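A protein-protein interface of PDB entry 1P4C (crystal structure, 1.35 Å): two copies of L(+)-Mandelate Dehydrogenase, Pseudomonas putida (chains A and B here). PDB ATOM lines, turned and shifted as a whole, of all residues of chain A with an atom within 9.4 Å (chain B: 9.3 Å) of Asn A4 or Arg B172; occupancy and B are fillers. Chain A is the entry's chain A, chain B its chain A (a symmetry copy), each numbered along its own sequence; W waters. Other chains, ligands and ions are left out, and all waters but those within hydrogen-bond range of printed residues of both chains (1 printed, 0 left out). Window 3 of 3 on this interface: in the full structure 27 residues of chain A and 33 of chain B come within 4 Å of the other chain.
Of chain B, only His B170 and Arg B172 come within 4 Å of Asn A4.
No residue of chain B comes within 4 Å of Leu A5.
Of the printed residues of chain B, Asn A7 touches Glu B166 (2.9 Å).
Of the printed residues of chain A, Tyr B164 touches Phe A6 (2.7 Å) and Leu A328 (3.8 Å).
Printed residues of chain A within 4 Å of Glu B166: Asn A7 (2.9 Å).
Of chain A, only Asn A4 and Phe A6 come within 4 Å of His B170.
Arg B172 touches just one residue of chain A: Asn A4 (2.6 Å).
The nearest printed residue of chain B that does not touch Phe A6 is Glu B166 (4.1 Å).
No position is printed for both chains.
Of the 7 pairs that touch across the chains among the printed residues, none has its exchanged pair printed and touching as well.
Among the printed residues, merely in contact across the chains: Phe A6 with His B170 (3.4 Å), Phe A6 with Leu B169 (3.5 Å), Asn A4 with His B170 (3.8 Å) and Leu A328 with Tyr B164 (3.8 Å).
Water W1 lies within hydrogen-bond range of a ring nitrogen (NE2) of His B170, the side-chain carboxylate (OD2) of Asp A10 and the side-chain amide nitrogen (ND2) of Asn A7.
O of Phe A6 is in hydrogen-bond range of OH of Tyr B164 (2.7 Å).
The side-chain carboxylate (OE2) of Glu B166 sits at hydrogen-bond distance from the side-chain amide nitrogen (ND2) of Asn A7 (2.9 Å).
OD1 of Asn A4 is in hydrogen-bond range of NH1 of Arg B172.
Of the 16 printed residues of chain B, 5 touch a printed residue of chain A.
Hydrophobic or aromatic side chains of chain B within 4 Å of the printed part of chain A: Tyr B164, Leu B169 and His B170.
Of the 17 printed residues of chain A, 4 touch a printed residue of chain B.
Hydrophobic or aromatic side chains of chain A that line the printed part of chain B: Phe A6 and Leu A328.
Along chain A the printed residues that touch a printed residue of chain B span positions 4 to 328.
Among the printed residues, 7 pairs touch across the chains.
Among the printed residues, no Asp or Glu carboxylate lies within 4 Å of a Lys or Arg side-chain nitrogen of the other chain.
The backbone carbonyl oxygen (O) of His B170 lies within hydrogen-bond range of the guanidinium group (NH1) of Arg B172 (2.8 Å).
N of Asp A10 sits at hydrogen-bond distance from OD1 of Asn A7 (2.8 Å).
The backbone NH (N) of Phe A6 is in hydrogen-bond range of the side-chain carboxylate (OD2) of Asp A10 (2.8 Å).
The backbone NH (N) of Glu A9 lies within hydrogen-bond range of the side-chain amide oxygen (OD1) of Asn A7 (3.0 Å).
NH1 of Arg B172 sits close to O of Leu B169 (3.3 Å).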
ATOM      1  N   ASN A   4      22.532 -27.554  18.963  1.00  0.00           N
ATOM      2  CA  ASN A   4      22.566 -27.944  17.524  1.00  0.00           C
ATOM      3  C   ASN A   4      23.529 -27.065  16.732  1.00  0.00           C
ATOM      4  O   ASN A   4      23.286 -25.873  16.548  1.00  0.00           O
ATOM      5  CB  ASN A   4      21.165 -27.839  16.915  1.00  0.00           C
ATOM      6  CG  ASN A   4      20.166 -28.760  17.587  1.00  0.00           C
ATOM      7  OD1 ASN A   4      20.359 -29.975  17.632  1.00  0.00           O
ATOM      8  ND2 ASN A   4      19.088 -28.186  18.110  1.00  0.00           N
ATOM      9  N   LEU A   5      24.626 -27.659  16.276  1.00  0.00           N
ATOM     10  CA  LEU A   5      25.621 -26.936  15.491  1.00  0.00           C
ATOM     11  C   LEU A   5      25.898 -27.745  14.229  1.00  0.00           C
ATOM     12  O   LEU A   5      26.899 -28.454  14.130  1.00  0.00           O
ATOM     13  CB  LEU A   5      26.902 -26.745  16.307  1.00  0.00           C
ATOM     14  CG  LEU A   5      26.733 -25.884  17.565  1.00  0.00           C
ATOM     15  CD1 LEU A   5      28.030 -25.864  18.361  1.00  0.00           C
ATOM     16  CD2 LEU A   5      26.326 -24.470  17.169  1.00  0.00           C
ATOM     17  N   PHE A   6      25.000 -27.619  13.257  1.00  0.00           N
ATOM     18  CA  PHE A   6      25.118 -28.370  12.017  1.00  0.00           C
ATOM     19  C   PHE A   6      25.376 -27.539  10.773  1.00  0.00           C
ATOM     20  O   PHE A   6      25.567 -28.088   9.693  1.00  0.00           O
ATOM     21  CB  PHE A   6      23.859 -29.215  11.822  1.00  0.00           C
ATOM     22  CG  PHE A   6      23.637 -30.216  12.918  1.00  0.00           C
ATOM     23  CD1 PHE A   6      24.487 -31.306  13.059  1.00  0.00           C
ATOM     24  CD2 PHE A   6      22.593 -30.057  13.822  1.00  0.00           C
ATOM     25  CE1 PHE A   6      24.307 -32.223  14.095  1.00  0.00           C
ATOM     26  CE2 PHE A   6      22.404 -30.968  14.862  1.00  0.00           C
ATOM     27  CZ  PHE A   6      23.262 -32.053  14.995  1.00  0.00           C
ATOM     28  N   ASN A   7      25.376 -26.219  10.918  1.00  0.00           N
ATOM     29  CA  ASN A   7      25.634 -25.336   9.790  1.00  0.00           C
ATOM     30  C   ASN A   7      26.061 -23.971  10.304  1.00  0.00           C
ATOM     31  O   ASN A   7      26.109 -23.746  11.512  1.00  0.00           O
ATOM     32  CB  ASN A   7      24.395 -25.213   8.893  1.00  0.00           C
ATOM     33  CG  ASN A   7      23.185 -24.687   9.633  1.00  0.00           C
ATOM     34  OD1 ASN A   7      23.282 -23.749  10.421  1.00  0.00           O
ATOM     35  ND2 ASN A   7      22.027 -25.281   9.368  1.00  0.00           N
ATOM     36  N   VAL A   8      26.373 -23.062   9.388  1.00  0.00           N
ATOM     37  CA  VAL A   8      26.817 -21.726   9.765  1.00  0.00           C
ATOM     38  C   VAL A   8      25.754 -20.942  10.540  1.00  0.00           C
ATOM     39  O   VAL A   8      26.077 -20.248  11.506  1.00  0.00           O
ATOM     40  CB  VAL A   8      27.269 -20.940   8.510  1.00  0.00           C
ATOM     41  CG1 VAL A   8      27.535 -19.487   8.856  1.00  0.00           C
ATOM     42  CG2 VAL A   8      28.532 -21.577   7.941  1.00  0.00           C
ATOM     43  N   GLU A   9      24.491 -21.056  10.136  1.00  0.00           N
ATOM     44  CA  GLU A   9      23.414 -20.349  10.832  1.00  0.00           C
ATOM     45  C   GLU A   9      23.342 -20.750  12.305  1.00  0.00           C
ATOM     46  O   GLU A   9      23.051 -19.918  13.166  1.00  0.00           O
ATOM     47  CB  GLU A   9      22.065 -20.620  10.152  1.00  0.00           C
ATOM     48  CG  GLU A   9      20.848 -20.125  10.936  1.00  0.00           C
ATOM     49  CD  GLU A   9      20.670 -18.615  10.918  1.00  0.00           C
ATOM     50  OE1 GLU A   9      21.609 -17.890  10.532  1.00  0.00           O
ATOM     51  OE2 GLU A   9      19.577 -18.148  11.300  1.00  0.00           O
ATOM     52  N   ASP A  10      23.603 -22.021  12.599  1.00  0.00           N
ATOM     53  CA  ASP A  10      23.573 -22.479  13.983  1.00  0.00           C
ATOM     54  C   ASP A  10      24.647 -21.762  14.791  1.00  0.00           C
ATOM     55  O   ASP A  10      24.441 -21.452  15.967  1.00  0.00           O
ATOM     56  CB  ASP A  10      23.784 -23.992  14.068  1.00  0.00           C
ATOM     57  CG  ASP A  10      22.596 -24.776  13.544  1.00  0.00           C
ATOM     58  OD1 ASP A  10      21.467 -24.241  13.566  1.00  0.00           O
ATOM     59  OD2 ASP A  10      22.788 -25.934  13.126  1.00  0.00           O
ATOM     60  N   TYR A  11      25.797 -21.503  14.172  1.00  0.00           N
ATOM     61  CA  TYR A  11      26.849 -20.789  14.878  1.00  0.00           C
ATOM     62  C   TYR A  11      26.480 -19.322  15.020  1.00  0.00           C
ATOM     63  O   TYR A  11      26.824 -18.693  16.019  1.00  0.00           O
ATOM     64  CB  TYR A  11      28.204 -20.953  14.180  1.00  0.00           C
ATOM     65  CG  TYR A  11      28.835 -22.290  14.487  1.00  0.00           C
ATOM     66  CD1 TYR A  11      28.447 -23.440  13.801  1.00  0.00           C
ATOM     67  CD2 TYR A  11      29.760 -22.421  15.523  1.00  0.00           C
ATOM     68  CE1 TYR A  11      28.957 -24.686  14.143  1.00  0.00           C
ATOM     69  CE2 TYR A  11      30.277 -23.669  15.874  1.00  0.00           C
ATOM     70  CZ  TYR A  11      29.867 -24.793  15.180  1.00  0.00           C
ATOM     71  OH  TYR A  11      30.348 -26.032  15.526  1.00  0.00           O
ATOM     72  N   ARG A  12      25.773 -18.765  14.040  1.00  0.00           N
ATOM     73  CA  ARG A  12      25.360 -17.373  14.165  1.00  0.00           C
ATOM     74  C   ARG A  12      24.459 -17.268  15.393  1.00  0.00           C
ATOM     75  O   ARG A  12      24.602 -16.356  16.203  1.00  0.00           O
ATOM     76  CB  ARG A  12      24.574 -16.891  12.943  1.00  0.00           C
ATOM     77  CG  ARG A  12      24.168 -15.421  13.072  1.00  0.00           C
ATOM     78  CD  ARG A  12      23.080 -15.011  12.083  1.00  0.00           C
ATOM     79  NE  ARG A  12      21.823 -15.726  12.309  1.00  0.00           N
ATOM     80  CZ  ARG A  12      21.052 -15.587  13.386  1.00  0.00           C
ATOM     81  NH1 ARG A  12      21.396 -14.751  14.357  1.00  0.00           N
ATOM     82  NH2 ARG A  12      19.933 -16.291  13.492  1.00  0.00           N
ATOM     83  N   LYS A  13      23.527 -18.208  15.520  1.00  0.00           N
ATOM     84  CA  LYS A  13      22.606 -18.214  16.652  1.00  0.00           C
ATOM     85  C   LYS A  13      23.347 -18.311  17.982  1.00  0.00           C
ATOM     86  O   LYS A  13      23.002 -17.620  18.940  1.00  0.00           O
ATOM     87  CB  LYS A  13      21.615 -19.375  16.525  1.00  0.00           C
ATOM     88  CG  LYS A  13      20.655 -19.231  15.354  1.00  0.00           C
ATOM     89  CD  LYS A  13      19.730 -20.434  15.236  1.00  0.00           C
ATOM     90  CE  LYS A  13      18.779 -20.273  14.059  1.00  0.00           C
ATOM     91  NZ  LYS A  13      17.925 -21.474  13.861  1.00  0.00           N
ATOM     92  N   LEU A  14      24.361 -19.168  18.046  1.00  0.00           N
ATOM     93  CA  LEU A  14      25.130 -19.324  19.275  1.00  0.00           C
ATOM     94  C   LEU A  14      25.959 -18.071  19.554  1.00  0.00           C
ATOM     95  O   LEU A  14      26.114 -17.664  20.707  1.00  0.00           O
ATOM     96  CB  LEU A  14      26.045 -20.550  19.184  1.00  0.00           C
ATOM     97  CG  LEU A  14      26.797 -20.917  20.467  1.00  0.00           C
ATOM     98  CD1 LEU A  14      25.812 -21.039  21.628  1.00  0.00           C
ATOM     99  CD2 LEU A  14      27.547 -22.224  20.265  1.00  0.00           C
ATOM    100  N   ALA A  15      26.488 -17.457  18.501  1.00  0.00           N
ATOM    101  CA  ALA A  15      27.282 -16.244  18.656  1.00  0.00           C
ATOM    102  C   ALA A  15      26.416 -15.121  19.215  1.00  0.00           C
ATOM    103  O   ALA A  15      26.855 -14.358  20.077  1.00  0.00           O
ATOM    104  CB  ALA A  15      27.880 -15.826  17.317  1.00  0.00           C
ATOM    105  N   LYS A  17      23.947 -15.381  21.153  1.00  0.00           N
ATOM    106  CA  LYS A  17      23.671 -15.641  22.561  1.00  0.00           C
ATOM    107  C   LYS A  17      24.864 -15.344  23.461  1.00  0.00           C
ATOM    108  O   LYS A  17      24.693 -15.008  24.629  1.00  0.00           O
ATOM    109  CB  LYS A  17      23.257 -17.098  22.771  1.00  0.00           C
ATOM    110  CG  LYS A  17      21.944 -17.484  22.116  1.00  0.00           C
ATOM    111  CD  LYS A  17      21.459 -18.842  22.605  1.00  0.00           C
ATOM    112  CE  LYS A  17      22.475 -19.938  22.332  1.00  0.00           C
ATOM    113  NZ  LYS A  17      22.002 -21.257  22.832  1.00  0.00           N
ATOM    114  N   ALA A 316      31.373 -17.705  18.900  1.00  0.00           N
ATOM    115  CA  ALA A 316      30.660 -18.716  19.662  1.00  0.00           C
ATOM    116  C   ALA A 316      31.551 -19.667  20.451  1.00  0.00           C
ATOM    117  O   ALA A 316      31.294 -19.926  21.630  1.00  0.00           O
ATOM    118  CB  ALA A 316      29.760 -19.522  18.727  1.00  0.00           C
ATOM    119  N   ARG A 317      32.599 -20.174  19.807  1.00  0.00           N
ATOM    120  CA  ARG A 317      33.471 -21.156  20.441  1.00  0.00           C
ATOM    121  C   ARG A 317      34.973 -21.022  20.191  1.00  0.00           C
ATOM    122  O   ARG A 317      35.703 -22.012  20.231  1.00  0.00           O
ATOM    123  CB  ARG A 317      32.996 -22.554  20.026  1.00  0.00           C
ATOM    124  CG  ARG A 317      31.646 -22.942  20.615  1.00  0.00           C
ATOM    125  CD  ARG A 317      31.042 -24.162  19.926  1.00  0.00           C
ATOM    126  NE  ARG A 317      31.952 -25.302  19.851  1.00  0.00           N
ATOM    127  CZ  ARG A 317      32.411 -25.978  20.900  1.00  0.00           C
ATOM    128  NH1 ARG A 317      32.053 -25.633  22.130  1.00  0.00           N
ATOM    129  NH2 ARG A 317      33.225 -27.009  20.717  1.00  0.00           N
ATOM    130  N   GLU A 324      35.406 -26.012  13.627  1.00  0.00           N
ATOM    131  CA  GLU A 324      34.134 -26.674  13.374  1.00  0.00           C
ATOM    132  C   GLU A 324      33.416 -26.110  12.160  1.00  0.00           C
ATOM    133  O   GLU A 324      32.863 -26.866  11.360  1.00  0.00           O
ATOM    134  CB  GLU A 324      33.245 -26.588  14.620  1.00  0.00           C
ATOM    135  CG  GLU A 324      33.874 -27.295  15.821  1.00  0.00           C
ATOM    136  CD  GLU A 324      33.107 -27.114  17.118  1.00  0.00           C
ATOM    137  OE1 GLU A 324      32.338 -26.138  17.239  1.00  0.00           O
ATOM    138  OE2 GLU A 324      33.293 -27.946  18.033  1.00  0.00           O
ATOM    139  N   LEU A 328      32.595 -28.184   8.810  1.00  0.00           N
ATOM    140  CA  LEU A 328      31.245 -28.296   8.264  1.00  0.00           C
ATOM    141  C   LEU A 328      31.193 -27.812   6.821  1.00  0.00           C
ATOM    142  O   LEU A 328      30.594 -28.462   5.965  1.00  0.00           O
ATOM    143  CB  LEU A 328      30.256 -27.481   9.101  1.00  0.00           C
ATOM    144  CG  LEU A 328      29.877 -28.060  10.468  1.00  0.00           C
ATOM    145  CD1 LEU A 328      29.068 -27.030  11.242  1.00  0.00           C
ATOM    146  CD2 LEU A 328      29.081 -29.349  10.290  1.00  0.00           C
ATOM    147  N   MET B  22       9.427 -36.777  15.422  1.00  0.00           N
ATOM    148  CA  MET B  22      10.637 -37.174  14.718  1.00  0.00           C
ATOM    149  C   MET B  22      10.371 -37.963  13.438  1.00  0.00           C
ATOM    150  O   MET B  22      11.123 -37.846  12.469  1.00  0.00           O
ATOM    151  CB  MET B  22      11.523 -37.988  15.653  1.00  0.00           C
ATOM    152  CG  MET B  22      12.438 -38.954  14.942  1.00  0.00           C
ATOM    153  SD  MET B  22      13.328 -40.094  16.030  1.00  0.00           S
ATOM    154  CE  MET B  22      13.461 -39.089  17.516  1.00  0.00           C
ATOM    155  N   ASP B  25       9.006 -35.482  10.898  1.00  0.00           N
ATOM    156  CA  ASP B  25      10.109 -34.673  10.377  1.00  0.00           C
ATOM    157  C   ASP B  25      10.931 -35.450   9.360  1.00  0.00           C
ATOM    158  O   ASP B  25      11.406 -34.894   8.372  1.00  0.00           O
ATOM    159  CB  ASP B  25      11.029 -34.195  11.507  1.00  0.00           C
ATOM    160  CG  ASP B  25      10.441 -33.043  12.294  1.00  0.00           C
ATOM    161  OD1 ASP B  25       9.568 -32.328  11.756  1.00  0.00           O
ATOM    162  OD2 ASP B  25      10.869 -32.840  13.450  1.00  0.00           O
ATOM    163  N   TYR B  26      11.107 -36.740   9.611  1.00  0.00           N
ATOM    164  CA  TYR B  26      11.859 -37.593   8.706  1.00  0.00           C
ATOM    165  C   TYR B  26      11.123 -37.707   7.366  1.00  0.00           C
ATOM    166  O   TYR B  26      11.742 -37.747   6.303  1.00  0.00           O
ATOM    167  CB  TYR B  26      12.037 -38.971   9.349  1.00  0.00           C
ATOM    168  CG  TYR B  26      11.989 -40.117   8.377  1.00  0.00           C
ATOM    169  CD1 TYR B  26      13.082 -40.425   7.569  1.00  0.00           C
ATOM    170  CD2 TYR B  26      10.829 -40.878   8.241  1.00  0.00           C
ATOM    171  CE1 TYR B  26      13.018 -41.465   6.645  1.00  0.00           C
ATOM    172  CE2 TYR B  26      10.755 -41.911   7.327  1.00  0.00           C
ATOM    173  CZ  TYR B  26      11.849 -42.203   6.531  1.00  0.00           C
ATOM    174  OH  TYR B  26      11.766 -43.229   5.626  1.00  0.00           O
ATOM    175  N   TYR B 164      21.829 -33.992   3.310  1.00  0.00           N
ATOM    176  CA  TYR B 164      22.011 -33.365   4.613  1.00  0.00           C
ATOM    177  C   TYR B 164      20.672 -32.827   5.101  1.00  0.00           C
ATOM    178  O   TYR B 164      20.354 -31.653   4.907  1.00  0.00           O
ATOM    179  CB  TYR B 164      23.024 -32.228   4.492  1.00  0.00           C
ATOM    180  CG  TYR B 164      23.708 -31.849   5.784  1.00  0.00           C
ATOM    181  CD1 TYR B 164      24.597 -32.724   6.408  1.00  0.00           C
ATOM    182  CD2 TYR B 164      23.498 -30.599   6.365  1.00  0.00           C
ATOM    183  CE1 TYR B 164      25.266 -32.360   7.573  1.00  0.00           C
ATOM    184  CE2 TYR B 164      24.160 -30.226   7.531  1.00  0.00           C
ATOM    185  CZ  TYR B 164      25.044 -31.110   8.127  1.00  0.00           C
ATOM    186  OH  TYR B 164      25.722 -30.731   9.264  1.00  0.00           O
ATOM    187  N   ARG B 165      19.881 -33.696   5.720  1.00  0.00           N
ATOM    188  CA  ARG B 165      18.574 -33.301   6.224  1.00  0.00           C
ATOM    189  C   ARG B 165      18.717 -32.935   7.692  1.00  0.00           C
ATOM    190  O   ARG B 165      18.833 -33.791   8.571  1.00  0.00           O
ATOM    191  CB  ARG B 165      17.569 -34.429   5.995  1.00  0.00           C
ATOM    192  CG  ARG B 165      17.364 -34.705   4.502  1.00  0.00           C
ATOM    193  CD  ARG B 165      16.044 -35.392   4.208  1.00  0.00           C
ATOM    194  NE  ARG B 165      16.047 -36.797   4.596  1.00  0.00           N
ATOM    195  CZ  ARG B 165      16.698 -37.754   3.943  1.00  0.00           C
ATOM    196  NH1 ARG B 165      17.406 -37.464   2.860  1.00  0.00           N
ATOM    197  NH2 ARG B 165      16.634 -39.006   4.374  1.00  0.00           N
ATOM    198  N   GLU B 166      18.707 -31.634   7.938  1.00  0.00           N
ATOM    199  CA  GLU B 166      18.918 -31.100   9.268  1.00  0.00           C
ATOM    200  C   GLU B 166      17.862 -31.397  10.326  1.00  0.00           C
ATOM    201  O   GLU B 166      18.176 -31.380  11.516  1.00  0.00           O
ATOM    202  CB  GLU B 166      19.227 -29.606   9.137  1.00  0.00           C
ATOM    203  CG  GLU B 166      20.428 -29.415   8.197  1.00  0.00           C
ATOM    204  CD  GLU B 166      20.781 -27.975   7.886  1.00  0.00           C
ATOM    205  OE1 GLU B 166      19.864 -27.142   7.752  1.00  0.00           O
ATOM    206  OE2 GLU B 166      21.988 -27.688   7.745  1.00  0.00           O
ATOM    207  N   ARG B 167      16.625 -31.688   9.927  1.00  0.00           N
ATOM    208  CA  ARG B 167      15.622 -32.026  10.936  1.00  0.00           C
ATOM    209  C   ARG B 167      16.061 -33.325  11.611  1.00  0.00           C
ATOM    210  O   ARG B 167      15.965 -33.465  12.831  1.00  0.00           O
ATOM    211  CB  ARG B 167      14.239 -32.247  10.321  1.00  0.00           C
ATOM    212  CG  ARG B 167      13.628 -31.042   9.650  1.00  0.00           C
ATOM    213  CD  ARG B 167      12.148 -31.286   9.415  1.00  0.00           C
ATOM    214  NE  ARG B 167      11.571 -30.304   8.504  1.00  0.00           N
ATOM    215  CZ  ARG B 167      10.271 -30.047   8.415  1.00  0.00           C
ATOM    216  NH1 ARG B 167       9.406 -30.696   9.188  1.00  0.00           N
ATOM    217  NH2 ARG B 167       9.834 -29.145   7.549  1.00  0.00           N
ATOM    218  N   ASP B 168      16.537 -34.277  10.813  1.00  0.00           N
ATOM    219  CA  ASP B 168      16.986 -35.562  11.345  1.00  0.00           C
ATOM    220  C   ASP B 168      18.179 -35.379  12.275  1.00  0.00           C
ATOM    221  O   ASP B 168      18.294 -36.065  13.290  1.00  0.00           O
ATOM    222  CB  ASP B 168      17.370 -36.519  10.210  1.00  0.00           C
ATOM    223  CG  ASP B 168      16.185 -36.921   9.346  1.00  0.00           C
ATOM    224  OD1 ASP B 168      15.028 -36.694   9.759  1.00  0.00           O
ATOM    225  OD2 ASP B 168      16.418 -37.481   8.254  1.00  0.00           O
ATOM    226  N   LEU B 169      19.075 -34.462  11.925  1.00  0.00           N
ATOM    227  CA  LEU B 169      20.245 -34.206  12.755  1.00  0.00           C
ATOM    228  C   LEU B 169      19.812 -33.620  14.097  1.00  0.00           C
ATOM    229  O   LEU B 169      20.351 -33.982  15.143  1.00  0.00           O
ATOM    230  CB  LEU B 169      21.207 -33.255  12.035  1.00  0.00           C
ATOM    231  CG  LEU B 169      21.812 -33.827  10.749  1.00  0.00           C
ATOM    232  CD1 LEU B 169      22.629 -32.759  10.041  1.00  0.00           C
ATOM    233  CD2 LEU B 169      22.682 -35.032  11.081  1.00  0.00           C
ATOM    234  N   HIS B 170      18.832 -32.724  14.070  1.00  0.00           N
ATOM    235  CA  HIS B 170      18.332 -32.118  15.301  1.00  0.00           C
ATOM    236  C   HIS B 170      17.642 -33.157  16.180  1.00  0.00           C
ATOM    237  O   HIS B 170      17.758 -33.121  17.406  1.00  0.00           O
ATOM    238  CB  HIS B 170      17.331 -31.002  14.993  1.00  0.00           C
ATOM    239  CG  HIS B 170      17.944 -29.794  14.357  1.00  0.00           C
ATOM    240  ND1 HIS B 170      17.211 -28.671  14.041  1.00  0.00           N
ATOM    241  CD2 HIS B 170      19.217 -29.533  13.977  1.00  0.00           C
ATOM    242  CE1 HIS B 170      18.007 -27.769  13.494  1.00  0.00           C
ATOM    243  NE2 HIS B 170      19.228 -28.268  13.445  1.00  0.00           N
ATOM    244  N   ASN B 171      16.916 -34.076  15.551  1.00  0.00           N
ATOM    245  CA  ASN B 171      16.198 -35.110  16.286  1.00  0.00           C
ATOM    246  C   ASN B 171      17.029 -36.362  16.546  1.00  0.00           C
ATOM    247  O   ASN B 171      16.546 -37.302  17.176  1.00  0.00           O
ATOM    248  CB  ASN B 171      14.926 -35.524  15.534  1.00  0.00           C
ATOM    249  CG  ASN B 171      13.971 -34.370  15.307  1.00  0.00           C
ATOM    250  OD1 ASN B 171      13.800 -33.507  16.165  1.00  0.00           O
ATOM    251  ND2 ASN B 171      13.323 -34.363  14.146  1.00  0.00           N
ATOM    252  N   ARG B 172      18.271 -36.379  16.070  1.00  0.00           N
ATOM    253  CA  ARG B 172      19.123 -37.552  16.246  1.00  0.00           C
ATOM    254  C   ARG B 172      18.349 -38.764  15.734  1.00  0.00           C
ATOM    255  O   ARG B 172      18.458 -39.865  16.275  1.00  0.00           O
ATOM    256  CB  ARG B 172      19.476 -37.750  17.724  1.00  0.00           C
ATOM    257  CG  ARG B 172      20.610 -36.871  18.235  1.00  0.00           C
ATOM    258  CD  ARG B 172      20.288 -35.390  18.136  1.00  0.00           C
ATOM    259  NE  ARG B 172      21.387 -34.569  18.640  1.00  0.00           N
ATOM    260  CZ  ARG B 172      21.388 -33.240  18.641  1.00  0.00           C
ATOM    261  NH1 ARG B 172      20.347 -32.571  18.164  1.00  0.00           N
ATOM    262  NH2 ARG B 172      22.433 -32.577  19.121  1.00  0.00           N
ATOM    263  N   PHE B 173      17.563 -38.542  14.685  1.00  0.00           N
ATOM    264  CA  PHE B 173      16.741 -39.587  14.086  1.00  0.00           C
ATOM    265  C   PHE B 173      17.479 -40.903  13.874  1.00  0.00           C
ATOM    266  O   PHE B 173      18.562 -40.935  13.291  1.00  0.00           O
ATOM    267  CB  PHE B 173      16.178 -39.113  12.743  1.00  0.00           C
ATOM    268  CG  PHE B 173      15.197 -40.071  12.127  1.00  0.00           C
ATOM    269  CD1 PHE B 173      13.954 -40.274  12.709  1.00  0.00           C
ATOM    270  CD2 PHE B 173      15.524 -40.788  10.984  1.00  0.00           C
ATOM    271  CE1 PHE B 173      13.041 -41.170  12.163  1.00  0.00           C
ATOM    272  CE2 PHE B 173      14.618 -41.691  10.426  1.00  0.00           C
ATOM    273  CZ  PHE B 173      13.374 -41.882  11.021  1.00  0.00           C
ATOM    274  N   LYS B 174      16.872 -41.986  14.348  1.00  0.00           N
ATOM    275  CA  LYS B 174      17.435 -43.324  14.211  1.00  0.00           C
ATOM    276  C   LYS B 174      16.368 -44.241  13.608  1.00  0.00           C
ATOM    277  O   LYS B 174      15.204 -44.190  14.019  1.00  0.00           O
ATOM    278  CB  LYS B 174      17.864 -43.856  15.585  1.00  0.00           C
ATOM    279  N   ILE B 175      16.758 -45.058  12.623  1.00  0.00           N
ATOM    280  CA  ILE B 175      15.827 -45.994  11.978  1.00  0.00           C
ATOM    281  C   ILE B 175      15.116 -46.778  13.084  1.00  0.00           C
ATOM    282  O   ILE B 175      15.758 -47.486  13.860  1.00  0.00           O
ATOM    283  CB  ILE B 175      16.578 -46.992  11.036  1.00  0.00           C
ATOM    284  CG1 ILE B 175      17.371 -46.228   9.977  1.00  0.00           C
ATOM    285  CG2 ILE B 175      15.588 -47.901  10.308  1.00  0.00           C
ATOM    286  CD1 ILE B 175      18.683 -46.858   9.667  1.00  0.00           C
ATOM    287  N   PRO B 176      13.783 -46.635  13.182  1.00  0.00           N
ATOM    288  CA  PRO B 176      12.958 -47.313  14.189  1.00  0.00           C
ATOM    289  C   PRO B 176      13.381 -48.758  14.427  1.00  0.00           C
ATOM    290  O   PRO B 176      13.619 -49.512  13.484  1.00  0.00           O
ATOM    291  CB  PRO B 176      11.555 -47.197  13.608  1.00  0.00           C
ATOM    292  CG  PRO B 176      11.599 -45.844  12.970  1.00  0.00           C
ATOM    293  CD  PRO B 176      12.939 -45.856  12.258  1.00  0.00           C
HETATM  294  O   HOH W   1      20.721 -27.068  11.771  1.00  0.00           O
